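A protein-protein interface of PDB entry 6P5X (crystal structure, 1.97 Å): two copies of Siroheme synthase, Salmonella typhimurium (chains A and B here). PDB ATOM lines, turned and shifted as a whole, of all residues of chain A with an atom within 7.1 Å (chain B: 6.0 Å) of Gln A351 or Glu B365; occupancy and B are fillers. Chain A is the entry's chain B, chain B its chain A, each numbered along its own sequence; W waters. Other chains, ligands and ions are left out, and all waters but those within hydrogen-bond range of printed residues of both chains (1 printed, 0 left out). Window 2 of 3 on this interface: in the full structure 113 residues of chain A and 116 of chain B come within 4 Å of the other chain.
The backbone NH (N) of Gln A351 sits at hydrogen-bond distance from the backbone carbonyl oxygen (O) of Lys A375 (2.8 Å). The indole nitrogen of Trp B368 is in hydrogen-bond range of the side-chain carboxylate of Glu B365 (3.4 Å). NZ of Lys A375 is in hydrogen-bond range of O of Asp A348 (3.0 Å). The backbone carbonyl oxygen (O) of Ser A352 lies within hydrogen-bond range of the backbone NH (N) of Thr A377, 3.1 Å away. OE2 of Glu B365 is in salt-bridge range of NZ of Lys B393 (3.7 Å).
Of chain B, only Phe B307 (3.9 Å), Val B356 (3.7 Å), Thr B357 (3.3 Å), Leu B360 (3.1 Å), Glu B365 (3.5 Å) and Leu B366 (3.8 Å) come within 4 Å of Gln A351. Printed residues of chain B within 4 Å of Ser A352: Leu B355. Thr A377 touches none of the printed residues of chain B. Printed residues of chain A within 4 Å of Glu B365: Gln A351. Of the printed residues of chain A, Leu B366 touches Gln A351. The nearest printed residue of chain A that does not touch Glu B365 is Lys A375 (7.1 Å).
OD2 of Asp A348 lies within salt-bridge range of NZ of Lys B361 (3.3 Å). N of Thr B357 lies within hydrogen-bond range of O of Gln A351, 3.3 Å away. The side-chain hydroxyl (OG1) of Thr A345 is in hydrogen-bond range of the backbone NH (N) of Phe B307, 2.8 Å away. N of Leu B355 is in hydrogen-bond range of O of Val A353, 2.8 Å away. The backbone carbonyl oxygen (O) of Glu B365 lies close to the side-chain amide oxygen (OE1) of Gln A351.
Among the printed residues, 10 pairs touch across the chains. Among the printed residues, Asp or Glu carboxylates within 4 Å of a Lys or Arg side-chain nitrogen of the other chain: Asp A348 with Lys B361 (3.3 Å).
Among the printed residues, merely in contact across the chains: Gln A351 with Phe B307, Gln A351 with Val B356, Gln A351 with Leu B360, Gln A351 with Leu B366 and Ser A352 with Leu B355.
Water W1 bridges the side-chain amide nitrogen of Gln A351 and the backbone NH of Asp B367.
No position is printed for both chains. Of the 10 pairs that touch across the chains among the printed residues, none has its exchanged pair printed and touching as well.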
ATOM      1  N   THR A 345      19.368  28.527  34.270  1.00  0.00           N
ATOM      2  CA  THR A 345      18.972  27.137  34.096  1.00  0.00           C
ATOM      3  C   THR A 345      18.174  26.697  35.317  1.00  0.00           C
ATOM      4  O   THR A 345      18.305  27.263  36.407  1.00  0.00           O
ATOM      5  CB  THR A 345      20.190  26.198  33.936  1.00  0.00           C
ATOM      6  OG1 THR A 345      20.949  26.215  35.145  1.00  0.00           O
ATOM      7  CG2 THR A 345      21.107  26.666  32.815  1.00  0.00           C
ATOM      8  N   ARG A 347      16.208  22.727  36.588  1.00  0.00           N
ATOM      9  CA  ARG A 347      15.678  21.392  36.323  1.00  0.00           C
ATOM     10  C   ARG A 347      15.924  21.096  34.844  1.00  0.00           C
ATOM     11  O   ARG A 347      17.039  21.313  34.352  1.00  0.00           O
ATOM     12  CB  ARG A 347      14.230  21.290  36.753  1.00  0.00           C
ATOM     13  CG  ARG A 347      13.972  21.783  38.182  1.00  0.00           C
ATOM     14  CD  ARG A 347      12.617  21.307  38.684  1.00  0.00           C
ATOM     15  NE  ARG A 347      12.769  20.175  39.583  1.00  0.00           N
ATOM     16  CZ  ARG A 347      12.700  20.267  40.904  1.00  0.00           C
ATOM     17  NH1 ARG A 347      12.454  21.438  41.471  1.00  0.00           N
ATOM     18  NH2 ARG A 347      12.872  19.196  41.656  1.00  0.00           N
ATOM     19  N   ASP A 348      14.922  20.648  34.097  1.00  0.00           N
ATOM     20  CA  ASP A 348      15.029  20.379  32.667  1.00  0.00           C
ATOM     21  C   ASP A 348      14.474  21.520  31.815  1.00  0.00           C
ATOM     22  O   ASP A 348      14.115  21.294  30.656  1.00  0.00           O
ATOM     23  CB  ASP A 348      14.305  19.071  32.333  1.00  0.00           C
ATOM     24  CG  ASP A 348      12.808  19.140  32.624  1.00  0.00           C
ATOM     25  OD1 ASP A 348      12.423  19.857  33.565  1.00  0.00           O
ATOM     26  OD2 ASP A 348      12.021  18.476  31.902  1.00  0.00           O
ATOM     27  N   TYR A 349      14.370  22.733  32.372  1.00  0.00           N
ATOM     28  CA  TYR A 349      13.805  23.838  31.604  1.00  0.00           C
ATOM     29  C   TYR A 349      14.663  24.165  30.390  1.00  0.00           C
ATOM     30  O   TYR A 349      14.132  24.443  29.308  1.00  0.00           O
ATOM     31  CB  TYR A 349      13.668  25.092  32.462  1.00  0.00           C
ATOM     32  CG  TYR A 349      12.531  25.089  33.446  1.00  0.00           C
ATOM     33  CD1 TYR A 349      11.939  23.911  33.874  1.00  0.00           C
ATOM     34  CD2 TYR A 349      12.031  26.283  33.929  1.00  0.00           C
ATOM     35  CE1 TYR A 349      10.883  23.928  34.787  1.00  0.00           C
ATOM     36  CE2 TYR A 349      10.986  26.314  34.835  1.00  0.00           C
ATOM     37  CZ  TYR A 349      10.420  25.141  35.264  1.00  0.00           C
ATOM     38  OH  TYR A 349       9.383  25.196  36.165  1.00  0.00           O
ATOM     39  N   ALA A 350      15.989  24.143  30.552  1.00  0.00           N
ATOM     40  CA  ALA A 350      16.916  24.612  29.529  1.00  0.00           C
ATOM     41  C   ALA A 350      18.127  23.691  29.459  1.00  0.00           C
ATOM     42  O   ALA A 350      18.800  23.468  30.469  1.00  0.00           O
ATOM     43  CB  ALA A 350      17.372  26.047  29.820  1.00  0.00           C
ATOM     44  N   GLN A 351      18.407  23.171  28.259  1.00  0.00           N
ATOM     45  CA  GLN A 351      19.661  22.461  28.011  1.00  0.00           C
ATOM     46  C   GLN A 351      20.806  23.414  27.711  1.00  0.00           C
ATOM     47  O   GLN A 351      21.972  23.020  27.818  1.00  0.00           O
ATOM     48  CB  GLN A 351      19.510  21.488  26.842  1.00  0.00           C
ATOM     49  CG  GLN A 351      18.458  20.409  27.049  1.00  0.00           C
ATOM     50  CD  GLN A 351      18.205  19.596  25.787  1.00  0.00           C
ATOM     51  OE1 GLN A 351      17.627  18.513  25.842  1.00  0.00           O
ATOM     52  NE2 GLN A 351      18.630  20.125  24.642  1.00  0.00           N
ATOM     53  N   SER A 352      20.506  24.645  27.319  1.00  0.00           N
ATOM     54  CA  SER A 352      21.569  25.604  27.070  1.00  0.00           C
ATOM     55  C   SER A 352      21.084  27.018  27.352  1.00  0.00           C
ATOM     56  O   SER A 352      19.887  27.315  27.287  1.00  0.00           O
ATOM     57  CB  SER A 352      22.091  25.496  25.634  1.00  0.00           C
ATOM     58  OG  SER A 352      21.054  25.695  24.693  1.00  0.00           O
ATOM     59  N   VAL A 353      22.036  27.882  27.676  1.00  0.00           N
ATOM     60  CA  VAL A 353      21.812  29.317  27.808  1.00  0.00           C
ATOM     61  C   VAL A 353      22.504  29.972  26.630  1.00  0.00           C
ATOM     62  O   VAL A 353      23.656  29.643  26.314  1.00  0.00           O
ATOM     63  CB  VAL A 353      22.377  29.856  29.134  1.00  0.00           C
ATOM     64  CG1 VAL A 353      22.073  31.336  29.271  1.00  0.00           C
ATOM     65  CG2 VAL A 353      21.832  29.018  30.324  1.00  0.00           C
ATOM     66  N   GLU A 374      13.334  25.036  21.124  1.00  0.00           N
ATOM     67  CA  GLU A 374      12.919  24.793  22.498  1.00  0.00           C
ATOM     68  C   GLU A 374      14.102  24.433  23.393  1.00  0.00           C
ATOM     69  O   GLU A 374      15.186  24.084  22.924  1.00  0.00           O
ATOM     70  CB  GLU A 374      11.899  23.655  22.545  1.00  0.00           C
ATOM     71  CG  GLU A 374      10.600  23.948  21.825  1.00  0.00           C
ATOM     72  CD  GLU A 374       9.648  22.763  21.853  1.00  0.00           C
ATOM     73  OE1 GLU A 374      10.016  21.717  22.432  1.00  0.00           O
ATOM     74  OE2 GLU A 374       8.533  22.879  21.297  1.00  0.00           O
ATOM     75  N   LYS A 375      13.861  24.518  24.709  1.00  0.00           N
ATOM     76  CA  LYS A 375      14.800  24.088  25.750  1.00  0.00           C
ATOM     77  C   LYS A 375      16.018  25.005  25.861  1.00  0.00           C
ATOM     78  O   LYS A 375      17.105  24.552  26.222  1.00  0.00           O
ATOM     79  CB  LYS A 375      15.256  22.640  25.538  1.00  0.00           C
ATOM     80  CG  LYS A 375      14.149  21.595  25.649  1.00  0.00           C
ATOM     81  CD  LYS A 375      13.280  21.867  26.864  1.00  0.00           C
ATOM     82  CE  LYS A 375      12.801  20.587  27.527  1.00  0.00           C
ATOM     83  NZ  LYS A 375      11.914  20.883  28.693  1.00  0.00           N
ATOM     84  N   GLN A 376      15.842  26.302  25.583  1.00  0.00           N
ATOM     85  CA  GLN A 376      16.887  27.302  25.739  1.00  0.00           C
ATOM     86  C   GLN A 376      16.402  28.414  26.652  1.00  0.00           C
ATOM     87  O   GLN A 376      15.202  28.686  26.734  1.00  0.00           O
ATOM     88  CB  GLN A 376      17.280  27.948  24.402  1.00  0.00           C
ATOM     89  CG  GLN A 376      17.607  27.010  23.259  1.00  0.00           C
ATOM     90  CD  GLN A 376      18.017  27.791  22.011  1.00  0.00           C
ATOM     91  OE1 GLN A 376      19.165  28.223  21.888  1.00  0.00           O
ATOM     92  NE2 GLN A 376      17.072  27.999  21.097  1.00  0.00           N
ATOM     93  N   THR A 377      17.354  29.062  27.322  1.00  0.00           N
ATOM     94  CA  THR A 377      17.181  30.395  27.885  1.00  0.00           C
ATOM     95  C   THR A 377      17.937  31.361  26.983  1.00  0.00           C
ATOM     96  O   THR A 377      19.164  31.238  26.828  1.00  0.00           O
ATOM     97  CB  THR A 377      17.720  30.475  29.320  1.00  0.00           C
ATOM     98  OG1 THR A 377      17.031  29.517  30.147  1.00  0.00           O
ATOM     99  CG2 THR A 377      17.530  31.891  29.901  1.00  0.00           C
ATOM    100  N   PHE B 307      23.665  25.962  35.805  1.00  0.00           N
ATOM    101  CA  PHE B 307      23.876  24.524  36.028  1.00  0.00           C
ATOM    102  C   PHE B 307      24.305  24.233  37.461  1.00  0.00           C
ATOM    103  O   PHE B 307      25.058  23.290  37.716  1.00  0.00           O
ATOM    104  CB  PHE B 307      24.891  23.925  35.044  1.00  0.00           C
ATOM    105  CG  PHE B 307      24.515  24.106  33.599  1.00  0.00           C
ATOM    106  CD1 PHE B 307      23.341  23.560  33.102  1.00  0.00           C
ATOM    107  CD2 PHE B 307      25.335  24.831  32.743  1.00  0.00           C
ATOM    108  CE1 PHE B 307      22.982  23.743  31.774  1.00  0.00           C
ATOM    109  CE2 PHE B 307      24.979  25.011  31.417  1.00  0.00           C
ATOM    110  CZ  PHE B 307      23.808  24.473  30.935  1.00  0.00           C
ATOM    111  N   LEU B 355      26.028  28.197  26.472  1.00  0.00           N
ATOM    112  CA  LEU B 355      26.481  27.457  27.649  1.00  0.00           C
ATOM    113  C   LEU B 355      25.621  26.198  27.688  1.00  0.00           C
ATOM    114  O   LEU B 355      24.415  26.287  27.893  1.00  0.00           O
ATOM    115  CB  LEU B 355      26.309  28.293  28.921  1.00  0.00           C
ATOM    116  CG  LEU B 355      26.971  29.683  28.909  1.00  0.00           C
ATOM    117  CD1 LEU B 355      26.939  30.318  30.296  1.00  0.00           C
ATOM    118  CD2 LEU B 355      28.393  29.608  28.416  1.00  0.00           C
ATOM    119  N   VAL B 356      26.235  25.037  27.467  1.00  0.00           N
ATOM    120  CA  VAL B 356      25.506  23.789  27.234  1.00  0.00           C
ATOM    121  C   VAL B 356      25.904  22.769  28.295  1.00  0.00           C
ATOM    122  O   VAL B 356      27.082  22.684  28.664  1.00  0.00           O
ATOM    123  CB  VAL B 356      25.819  23.201  25.837  1.00  0.00           C
ATOM    124  CG1 VAL B 356      24.830  22.092  25.491  1.00  0.00           C
ATOM    125  CG2 VAL B 356      25.844  24.282  24.776  1.00  0.00           C
ATOM    126  N   THR B 357      24.942  21.969  28.746  1.00  0.00           N
ATOM    127  CA  THR B 357      25.274  20.838  29.604  1.00  0.00           C
ATOM    128  C   THR B 357      25.590  19.612  28.752  1.00  0.00           C
ATOM    129  O   THR B 357      24.802  19.231  27.879  1.00  0.00           O
ATOM    130  CB  THR B 357      24.152  20.524  30.599  1.00  0.00           C
ATOM    131  OG1 THR B 357      24.495  19.333  31.318  1.00  0.00           O
ATOM    132  CG2 THR B 357      22.782  20.333  29.907  1.00  0.00           C
ATOM    133  N   LEU B 360      23.157  15.114  30.216  1.00  0.00           N
ATOM    134  CA  LEU B 360      21.730  15.360  30.090  1.00  0.00           C
ATOM    135  C   LEU B 360      20.920  14.209  30.678  1.00  0.00           C
ATOM    136  O   LEU B 360      21.436  13.116  30.929  1.00  0.00           O
ATOM    137  CB  LEU B 360      21.352  15.581  28.620  1.00  0.00           C
ATOM    138  CG  LEU B 360      20.004  16.241  28.333  1.00  0.00           C
ATOM    139  CD1 LEU B 360      19.782  17.423  29.271  1.00  0.00           C
ATOM    140  CD2 LEU B 360      19.941  16.677  26.884  1.00  0.00           C
ATOM    141  N   LYS B 361      19.632  14.488  30.898  1.00  0.00           N
ATOM    142  CA  LYS B 361      18.704  13.513  31.458  1.00  0.00           C
ATOM    143  C   LYS B 361      18.719  12.223  30.647  1.00  0.00           C
ATOM    144  O   LYS B 361      18.959  12.229  29.436  1.00  0.00           O
ATOM    145  CB  LYS B 361      17.288  14.098  31.497  1.00  0.00           C
ATOM    146  CG  LYS B 361      16.353  13.413  32.484  1.00  0.00           C
ATOM    147  CD  LYS B 361      14.891  13.643  32.123  1.00  0.00           C
ATOM    148  CE  LYS B 361      14.590  15.116  31.876  1.00  0.00           C
ATOM    149  NZ  LYS B 361      13.141  15.358  31.613  1.00  0.00           N
ATOM    150  N   GLY B 363      16.962  10.028  29.032  1.00  0.00           N
ATOM    151  CA  GLY B 363      16.470   9.888  27.674  1.00  0.00           C
ATOM    152  C   GLY B 363      16.668  11.121  26.815  1.00  0.00           C
ATOM    153  O   GLY B 363      16.441  11.085  25.600  1.00  0.00           O
ATOM    154  N   GLY B 364      17.097  12.219  27.435  1.00  0.00           N
ATOM    155  CA  GLY B 364      17.263  13.457  26.701  1.00  0.00           C
ATOM    156  C   GLY B 364      18.402  13.387  25.703  1.00  0.00           C
ATOM    157  O   GLY B 364      19.361  12.630  25.858  1.00  0.00           O
ATOM    158  N   GLU B 365      18.279  14.186  24.648  1.00  0.00           N
ATOM    159  CA  GLU B 365      19.332  14.350  23.659  1.00  0.00           C
ATOM    160  C   GLU B 365      19.457  15.825  23.307  1.00  0.00           C
ATOM    161  O   GLU B 365      18.449  16.515  23.125  1.00  0.00           O
ATOM    162  CB  GLU B 365      19.064  13.529  22.388  1.00  0.00           C
ATOM    163  CG  GLU B 365      20.007  13.873  21.237  1.00  0.00           C
ATOM    164  CD  GLU B 365      20.195  12.732  20.254  1.00  0.00           C
ATOM    165  OE1 GLU B 365      19.183  12.199  19.754  1.00  0.00           O
ATOM    166  OE2 GLU B 365      21.360  12.365  19.987  1.00  0.00           O
ATOM    167  N   LEU B 366      20.696  16.302  23.228  1.00  0.00           N
ATOM    168  CA  LEU B 366      20.962  17.679  22.832  1.00  0.00           C
ATOM    169  C   LEU B 366      20.515  17.910  21.391  1.00  0.00           C
ATOM    170  O   LEU B 366      20.396  16.980  20.586  1.00  0.00           O
ATOM    171  CB  LEU B 366      22.447  18.011  22.977  1.00  0.00           C
ATOM    172  CG  LEU B 366      23.032  18.087  24.385  1.00  0.00           C
ATOM    173  CD1 LEU B 366      24.520  18.380  24.330  1.00  0.00           C
ATOM    174  CD2 LEU B 366      22.309  19.149  25.205  1.00  0.00           C
ATOM    175  N   ASP B 367      20.273  19.180  21.068  1.00  0.00           N
ATOM    176  CA  ASP B 367      19.727  19.566  19.768  1.00  0.00           C
ATOM    177  C   ASP B 367      20.895  19.875  18.839  1.00  0.00           C
ATOM    178  O   ASP B 367      21.306  21.027  18.665  1.00  0.00           O
ATOM    179  CB  ASP B 367      18.790  20.752  19.927  1.00  0.00           C
ATOM    180  CG  ASP B 367      17.990  21.023  18.687  1.00  0.00           C
ATOM    181  OD1 ASP B 367      18.240  20.374  17.654  1.00  0.00           O
ATOM    182  OD2 ASP B 367      17.099  21.891  18.749  1.00  0.00           O
ATOM    183  N   TRP B 368      21.436  18.825  18.221  1.00  0.00           N
ATOM    184  CA  TRP B 368      22.725  18.963  17.552  1.00  0.00           C
ATOM    185  C   TRP B 368      22.640  19.880  16.336  1.00  0.00           C
ATOM    186  O   TRP B 368      23.571  20.652  16.082  1.00  0.00           O
ATOM    187  CB  TRP B 368      23.259  17.577  17.182  1.00  0.00           C
ATOM    188  CG  TRP B 368      23.519  16.727  18.406  1.00  0.00           C
ATOM    189  CD1 TRP B 368      22.823  15.621  18.804  1.00  0.00           C
ATOM    190  CD2 TRP B 368      24.538  16.938  19.396  1.00  0.00           C
ATOM    191  NE1 TRP B 368      23.355  15.127  19.976  1.00  0.00           N
ATOM    192  CE2 TRP B 368      24.409  15.914  20.356  1.00  0.00           C
ATOM    193  CE3 TRP B 368      25.555  17.890  19.558  1.00  0.00           C
ATOM    194  CZ2 TRP B 368      25.248  15.818  21.462  1.00  0.00           C
ATOM    195  CZ3 TRP B 368      26.399  17.785  20.661  1.00  0.00           C
ATOM    196  CH2 TRP B 368      26.234  16.761  21.595  1.00  0.00           C
ATOM    197  N   LYS B 393      28.634  14.060  16.703  1.00  0.00           N
ATOM    198  CA  LYS B 393      27.364  14.711  16.418  1.00  0.00           C
ATOM    199  C   LYS B 393      27.569  16.067  15.749  1.00  0.00           C
ATOM    200  O   LYS B 393      26.853  16.403  14.802  1.00  0.00           O
ATOM    201  CB  LYS B 393      26.544  14.855  17.704  1.00  0.00           C
ATOM    202  CG  LYS B 393      26.073  13.527  18.299  1.00  0.00           C
ATOM    203  CD  LYS B 393      24.984  12.894  17.470  1.00  0.00           C
ATOM    204  CE  LYS B 393      24.539  11.559  18.044  1.00  0.00           C
ATOM    205  NZ  LYS B 393      23.425  11.002  17.237  1.00  0.00           N
HETATM  206  O   HOH W   1      20.148  21.117  22.999  1.00  0.00           O
